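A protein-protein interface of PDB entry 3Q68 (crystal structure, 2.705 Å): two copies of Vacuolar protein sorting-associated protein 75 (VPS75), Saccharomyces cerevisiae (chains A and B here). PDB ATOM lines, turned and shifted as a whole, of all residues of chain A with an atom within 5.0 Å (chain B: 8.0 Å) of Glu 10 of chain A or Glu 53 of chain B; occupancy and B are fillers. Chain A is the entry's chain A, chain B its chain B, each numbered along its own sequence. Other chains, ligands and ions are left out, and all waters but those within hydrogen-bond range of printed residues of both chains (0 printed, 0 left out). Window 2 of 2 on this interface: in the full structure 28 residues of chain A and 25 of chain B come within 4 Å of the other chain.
No position is printed for both chains.
Glu 10 of chain A touches just one residue of chain B: Glu 53. Of chain A, only Glu 10 and His 11 come within 4 Å of Glu 53 of chain B. Printed residues of chain B within 4 Å of His 11 of chain A: Glu 53. Printed residues of chain B within 4 Å of Lys 13 of chain A: Tyr 50 (3.95 Å). Printed residues of chain B within 4 Å of Ala 14 of chain A: Tyr 50. Of the printed residues of chain A, Tyr 50 of chain B touches Lys 13 (3.95 Å) and Ala 14 (3.5 Å). Tyr 216 of chain B touches none of the printed residues of chain A. The nearest printed residue of chain B that does not touch Lys 13 of chain A is Glu 53 of chain B (6.6 Å).
Hydrophobic or aromatic side chains of chain A within 4 Å of the printed part of chain B: His 11 and Ala 14. Of the 13 printed residues of chain B, 2 touch a printed residue of chain A. Hydrophobic or aromatic side chains of chain B within 4 Å of the printed part of chain A: Tyr 50. Among the printed residues, 4 pairs touch across the chains.
A ring nitrogen (NE2) of His 11 of chain A sits at hydrogen-bond distance from the backbone carbonyl oxygen (O) of Glu 53 of chain B (2.7 Å).
Glu 10 of chain A touches Glu 53 of chain B (CG to CG, 3.8 Å). Tyr 50 of chain B touches Lys 13 of chain A (CE1 to O, 3.95 Å). Tyr 50 of chain B touches Ala 14 of chain A (CD1 to CA, 3.5 Å).
The side-chain carboxylate (OE1) of Glu 10 of chain A is in salt-bridge range of the side-chain amino group (NZ) of Lys 13 of chain A, 3.6 Å away.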
ATOM      1  N   GLU A   8      -5.375  -5.021   6.734  1.00  0.00           N
ATOM      2  CA  GLU A   8      -6.789  -4.742   6.926  1.00  0.00           C
ATOM      3  C   GLU A   8      -7.127  -3.372   6.403  1.00  0.00           C
ATOM      4  O   GLU A   8      -8.007  -3.217   5.586  1.00  0.00           O
ATOM      5  CB  GLU A   8      -7.160  -4.793   8.406  1.00  0.00           C
ATOM      6  CG  GLU A   8      -8.612  -4.411   8.679  1.00  0.00           C
ATOM      7  CD  GLU A   8      -8.931  -4.306  10.154  1.00  0.00           C
ATOM      8  OE1 GLU A   8      -9.692  -3.398  10.535  1.00  0.00           O
ATOM      9  OE2 GLU A   8      -8.444  -5.144  10.931  1.00  0.00           O
ATOM     10  N   ASN A   9      -6.427  -2.370   6.901  1.00  0.00           N
ATOM     11  CA  ASN A   9      -6.658  -1.007   6.478  1.00  0.00           C
ATOM     12  C   ASN A   9      -6.343  -0.814   5.009  1.00  0.00           C
ATOM     13  O   ASN A   9      -7.038  -0.094   4.306  1.00  0.00           O
ATOM     14  CB  ASN A   9      -5.837  -0.045   7.317  1.00  0.00           C
ATOM     15  CG  ASN A   9      -6.252   1.374   7.117  1.00  0.00           C
ATOM     16  OD1 ASN A   9      -7.416   1.648   6.848  1.00  0.00           O
ATOM     17  ND2 ASN A   9      -5.305   2.295   7.241  1.00  0.00           N
ATOM     18  N   GLU A  10      -5.274  -1.441   4.549  1.00  0.00           N
ATOM     19  CA  GLU A  10      -4.887  -1.336   3.156  1.00  0.00           C
ATOM     20  C   GLU A  10      -5.965  -1.970   2.307  1.00  0.00           C
ATOM     21  O   GLU A  10      -6.298  -1.502   1.226  1.00  0.00           O
ATOM     22  CB  GLU A  10      -3.567  -2.033   2.916  1.00  0.00           C
ATOM     23  CG  GLU A  10      -3.029  -1.780   1.543  1.00  0.00           C
ATOM     24  CD  GLU A  10      -2.790  -0.316   1.300  1.00  0.00           C
ATOM     25  OE1 GLU A  10      -3.387   0.229   0.354  1.00  0.00           O
ATOM     26  OE2 GLU A  10      -2.017   0.290   2.065  1.00  0.00           O
ATOM     27  N   HIS A  11      -6.494  -3.068   2.811  1.00  0.00           N
ATOM     28  CA  HIS A  11      -7.547  -3.774   2.126  1.00  0.00           C
ATOM     29  C   HIS A  11      -8.776  -2.903   2.043  1.00  0.00           C
ATOM     30  O   HIS A  11      -9.444  -2.860   1.040  1.00  0.00           O
ATOM     31  CB  HIS A  11      -7.863  -5.074   2.849  1.00  0.00           C
ATOM     32  CG  HIS A  11      -7.061  -6.236   2.358  1.00  0.00           C
ATOM     33  ND1 HIS A  11      -7.592  -7.497   2.208  1.00  0.00           N
ATOM     34  CD2 HIS A  11      -5.773  -6.321   1.954  1.00  0.00           C
ATOM     35  CE1 HIS A  11      -6.661  -8.314   1.752  1.00  0.00           C
ATOM     36  NE2 HIS A  11      -5.549  -7.622   1.584  1.00  0.00           N
ATOM     37  N   ALA A  12      -9.076  -2.201   3.114  1.00  0.00           N
ATOM     38  CA  ALA A  12     -10.226  -1.343   3.127  1.00  0.00           C
ATOM     39  C   ALA A  12     -10.017  -0.273   2.098  1.00  0.00           C
ATOM     40  O   ALA A  12     -10.918   0.094   1.375  1.00  0.00           O
ATOM     41  CB  ALA A  12     -10.380  -0.731   4.470  1.00  0.00           C
ATOM     42  N   LYS A  13      -8.806   0.232   2.024  1.00  0.00           N
ATOM     43  CA  LYS A  13      -8.522   1.278   1.074  1.00  0.00           C
ATOM     44  C   LYS A  13      -8.788   0.784  -0.322  1.00  0.00           C
ATOM     45  O   LYS A  13      -9.425   1.456  -1.116  1.00  0.00           O
ATOM     46  CB  LYS A  13      -7.062   1.664   1.215  1.00  0.00           C
ATOM     47  CG  LYS A  13      -6.423   2.179  -0.032  1.00  0.00           C
ATOM     48  CD  LYS A  13      -6.531   3.673  -0.115  1.00  0.00           C
ATOM     49  CE  LYS A  13      -5.169   4.289  -0.346  1.00  0.00           C
ATOM     50  NZ  LYS A  13      -4.279   3.411  -1.140  1.00  0.00           N
ATOM     51  N   ALA A  14      -8.327  -0.416  -0.616  1.00  0.00           N
ATOM     52  CA  ALA A  14      -8.545  -0.976  -1.930  1.00  0.00           C
ATOM     53  C   ALA A  14     -10.004  -1.200  -2.215  1.00  0.00           C
ATOM     54  O   ALA A  14     -10.479  -0.892  -3.277  1.00  0.00           O
ATOM     55  CB  ALA A  14      -7.815  -2.254  -2.051  1.00  0.00           C
ATOM     56  N   ARG B  47      -8.224   0.511 -11.318  1.00  0.00           N
ATOM     57  CA  ARG B  47      -8.855  -0.639 -10.718  1.00  0.00           C
ATOM     58  C   ARG B  47      -7.969  -1.842 -10.479  1.00  0.00           C
ATOM     59  O   ARG B  47      -8.068  -2.480  -9.456  1.00  0.00           O
ATOM     60  CB  ARG B  47     -10.037  -1.064 -11.561  1.00  0.00           C
ATOM     61  CG  ARG B  47     -10.315  -2.520 -11.469  1.00  0.00           C
ATOM     62  CD  ARG B  47     -11.349  -2.961 -12.466  1.00  0.00           C
ATOM     63  NE  ARG B  47     -10.915  -4.062 -13.312  1.00  0.00           N
ATOM     64  CZ  ARG B  47     -11.729  -4.924 -13.899  1.00  0.00           C
ATOM     65  NH1 ARG B  47     -13.034  -4.861 -13.729  1.00  0.00           N
ATOM     66  NH2 ARG B  47     -11.231  -5.868 -14.649  1.00  0.00           N
ATOM     67  N   ASP B  48      -7.115  -2.177 -11.428  1.00  0.00           N
ATOM     68  CA  ASP B  48      -6.235  -3.325 -11.275  1.00  0.00           C
ATOM     69  C   ASP B  48      -5.262  -3.039 -10.142  1.00  0.00           C
ATOM     70  O   ASP B  48      -5.063  -3.862  -9.254  1.00  0.00           O
ATOM     71  CB  ASP B  48      -5.556  -3.629 -12.596  1.00  0.00           C
ATOM     72  CG  ASP B  48      -6.541  -4.064 -13.652  1.00  0.00           C
ATOM     73  OD1 ASP B  48      -7.697  -4.330 -13.300  1.00  0.00           O
ATOM     74  OD2 ASP B  48      -6.168  -4.143 -14.831  1.00  0.00           O
ATOM     75  N   ALA B  49      -4.676  -1.852 -10.160  1.00  0.00           N
ATOM     76  CA  ALA B  49      -3.757  -1.456  -9.094  1.00  0.00           C
ATOM     77  C   ALA B  49      -4.319  -1.660  -7.675  1.00  0.00           C
ATOM     78  O   ALA B  49      -3.569  -1.919  -6.749  1.00  0.00           O
ATOM     79  CB  ALA B  49      -3.309  -0.013  -9.307  1.00  0.00           C
ATOM     80  N   TYR B  50      -5.632  -1.541  -7.507  1.00  0.00           N
ATOM     81  CA  TYR B  50      -6.264  -1.857  -6.230  1.00  0.00           C
ATOM     82  C   TYR B  50      -6.373  -3.363  -6.016  1.00  0.00           C
ATOM     83  O   TYR B  50      -6.394  -3.830  -4.875  1.00  0.00           O
ATOM     84  CB  TYR B  50      -7.679  -1.270  -6.137  1.00  0.00           C
ATOM     85  CG  TYR B  50      -7.775   0.225  -5.903  1.00  0.00           C
ATOM     86  CD1 TYR B  50      -7.376   0.796  -4.695  1.00  0.00           C
ATOM     87  CD2 TYR B  50      -8.300   1.063  -6.884  1.00  0.00           C
ATOM     88  CE1 TYR B  50      -7.479   2.163  -4.485  1.00  0.00           C
ATOM     89  CE2 TYR B  50      -8.407   2.425  -6.685  1.00  0.00           C
ATOM     90  CZ  TYR B  50      -8.000   2.976  -5.487  1.00  0.00           C
ATOM     91  OH  TYR B  50      -8.116   4.342  -5.298  1.00  0.00           O
ATOM     92  N   ILE B  51      -6.465  -4.121  -7.109  1.00  0.00           N
ATOM     93  CA  ILE B  51      -6.769  -5.555  -7.023  1.00  0.00           C
ATOM     94  C   ILE B  51      -5.633  -6.398  -6.433  1.00  0.00           C
ATOM     95  O   ILE B  51      -5.884  -7.376  -5.724  1.00  0.00           O
ATOM     96  CB  ILE B  51      -7.230  -6.149  -8.386  1.00  0.00           C
ATOM     97  CG1 ILE B  51      -8.587  -5.575  -8.798  1.00  0.00           C
ATOM     98  CG2 ILE B  51      -7.331  -7.668  -8.312  1.00  0.00           C
ATOM     99  CD1 ILE B  51      -9.260  -6.333  -9.932  1.00  0.00           C
ATOM    100  N   ASP B  52      -4.391  -6.022  -6.715  1.00  0.00           N
ATOM    101  CA  ASP B  52      -3.252  -6.773  -6.196  1.00  0.00           C
ATOM    102  C   ASP B  52      -3.338  -6.815  -4.687  1.00  0.00           C
ATOM    103  O   ASP B  52      -3.173  -7.871  -4.072  1.00  0.00           O
ATOM    104  CB  ASP B  52      -1.940  -6.125  -6.615  1.00  0.00           C
ATOM    105  CG  ASP B  52      -1.795  -6.063  -8.109  1.00  0.00           C
ATOM    106  OD1 ASP B  52      -2.829  -5.869  -8.788  1.00  0.00           O
ATOM    107  OD2 ASP B  52      -0.660  -6.214  -8.606  1.00  0.00           O
ATOM    108  N   GLU B  53      -3.614  -5.653  -4.104  1.00  0.00           N
ATOM    109  CA  GLU B  53      -3.761  -5.516  -2.664  1.00  0.00           C
ATOM    110  C   GLU B  53      -4.719  -6.544  -2.088  1.00  0.00           C
ATOM    111  O   GLU B  53      -4.683  -6.825  -0.886  1.00  0.00           O
ATOM    112  CB  GLU B  53      -4.225  -4.106  -2.306  1.00  0.00           C
ATOM    113  CG  GLU B  53      -3.092  -3.152  -1.985  1.00  0.00           C
ATOM    114  CD  GLU B  53      -2.017  -3.140  -3.056  1.00  0.00           C
ATOM    115  OE1 GLU B  53      -0.821  -3.033  -2.695  1.00  0.00           O
ATOM    116  OE2 GLU B  53      -2.367  -3.246  -4.253  1.00  0.00           O
ATOM    117  N   ILE B  54      -5.534  -7.143  -2.930  1.00  0.00           N
ATOM    118  CA  ILE B  54      -6.446  -8.142  -2.421  1.00  0.00           C
ATOM    119  C   ILE B  54      -5.919  -9.521  -2.778  1.00  0.00           C
ATOM    120  O   ILE B  54      -5.753  -9.846  -3.936  1.00  0.00           O
ATOM    121  CB  ILE B  54      -7.811  -7.946  -3.005  1.00  0.00           C
ATOM    122  CG1 ILE B  54      -8.120  -6.467  -3.042  1.00  0.00           C
ATOM    123  CG2 ILE B  54      -8.835  -8.662  -2.185  1.00  0.00           C
ATOM    124  CD1 ILE B  54      -9.377  -6.159  -3.723  1.00  0.00           C
ATOM    125  N   ALA B  55      -5.654 -10.333  -1.771  1.00  0.00           N
ATOM    126  CA  ALA B  55      -5.141 -11.664  -2.006  1.00  0.00           C
ATOM    127  C   ALA B  55      -6.190 -12.611  -2.512  1.00  0.00           C
ATOM    128  O   ALA B  55      -7.288 -12.656  -1.993  1.00  0.00           O
ATOM    129  CB  ALA B  55      -4.554 -12.210  -0.750  1.00  0.00           C
ATOM    130  N   GLU B  56      -5.854 -13.376  -3.536  1.00  0.00           N
ATOM    131  CA  GLU B  56      -6.790 -14.337  -4.083  1.00  0.00           C
ATOM    132  C   GLU B  56      -8.021 -13.718  -4.646  1.00  0.00           C
ATOM    133  O   GLU B  56      -9.066 -14.344  -4.695  1.00  0.00           O
ATOM    134  CB  GLU B  56      -7.226 -15.254  -2.968  1.00  0.00           C
ATOM    135  CG  GLU B  56      -6.277 -15.220  -1.818  1.00  0.00           C
ATOM    136  CD  GLU B  56      -6.283 -16.503  -1.039  1.00  0.00           C
ATOM    137  OE1 GLU B  56      -7.376 -16.972  -0.666  1.00  0.00           O
ATOM    138  OE2 GLU B  56      -5.190 -17.042  -0.800  1.00  0.00           O
ATOM    139  N   PHE B  57      -7.926 -12.490  -5.086  1.00  0.00           N
ATOM    140  CA  PHE B  57      -9.109 -11.905  -5.620  1.00  0.00           C
ATOM    141  C   PHE B  57      -9.527 -12.724  -6.810  1.00  0.00           C
ATOM    142  O   PHE B  57     -10.668 -13.150  -6.930  1.00  0.00           O
ATOM    143  CB  PHE B  57      -8.736 -10.509  -6.078  1.00  0.00           C
ATOM    144  CG  PHE B  57      -9.790  -9.822  -6.861  1.00  0.00           C
ATOM    145  CD1 PHE B  57     -10.851  -9.232  -6.239  1.00  0.00           C
ATOM    146  CD2 PHE B  57      -9.703  -9.735  -8.216  1.00  0.00           C
ATOM    147  CE1 PHE B  57     -11.796  -8.594  -6.958  1.00  0.00           C
ATOM    148  CE2 PHE B  57     -10.653  -9.099  -8.922  1.00  0.00           C
ATOM    149  CZ  PHE B  57     -11.694  -8.529  -8.294  1.00  0.00           C
ATOM    150  N   ASP B  84      -2.935 -14.853  -9.915  1.00  0.00           N
ATOM    151  CA  ASP B  84      -2.979 -13.734  -8.993  1.00  0.00           C
ATOM    152  C   ASP B  84      -3.027 -12.424  -9.753  1.00  0.00           C
ATOM    153  O   ASP B  84      -2.994 -11.355  -9.156  1.00  0.00           O
ATOM    154  CB  ASP B  84      -1.801 -13.784  -7.998  1.00  0.00           C
ATOM    155  CG  ASP B  84      -0.434 -13.710  -8.679  1.00  0.00           C
ATOM    156  OD1 ASP B  84      -0.375 -13.696  -9.927  1.00  0.00           O
ATOM    157  OD2 ASP B  84       0.593 -13.665  -7.954  1.00  0.00           O
ATOM    158  N   TYR B 216     -16.546 -10.667  -7.159  1.00  0.00           N
ATOM    159  CA  TYR B 216     -15.863 -10.777  -5.893  1.00  0.00           C
ATOM    160  C   TYR B 216     -16.815 -10.469  -4.770  1.00  0.00           C
ATOM    161  O   TYR B 216     -16.817 -11.106  -3.733  1.00  0.00           O
ATOM    162  CB  TYR B 216     -14.713  -9.792  -5.853  1.00  0.00           C
ATOM    163  CG  TYR B 216     -13.864  -9.936  -4.638  1.00  0.00           C
ATOM    164  CD1 TYR B 216     -13.033 -11.014  -4.485  1.00  0.00           C
ATOM    165  CD2 TYR B 216     -13.899  -8.999  -3.639  1.00  0.00           C
ATOM    166  CE1 TYR B 216     -12.262 -11.151  -3.376  1.00  0.00           C
ATOM    167  CE2 TYR B 216     -13.132  -9.123  -2.529  1.00  0.00           C
ATOM    168  CZ  TYR B 216     -12.314 -10.201  -2.394  1.00  0.00           C
ATOM    169  OH  TYR B 216     -11.540 -10.329  -1.272  1.00  0.00           O
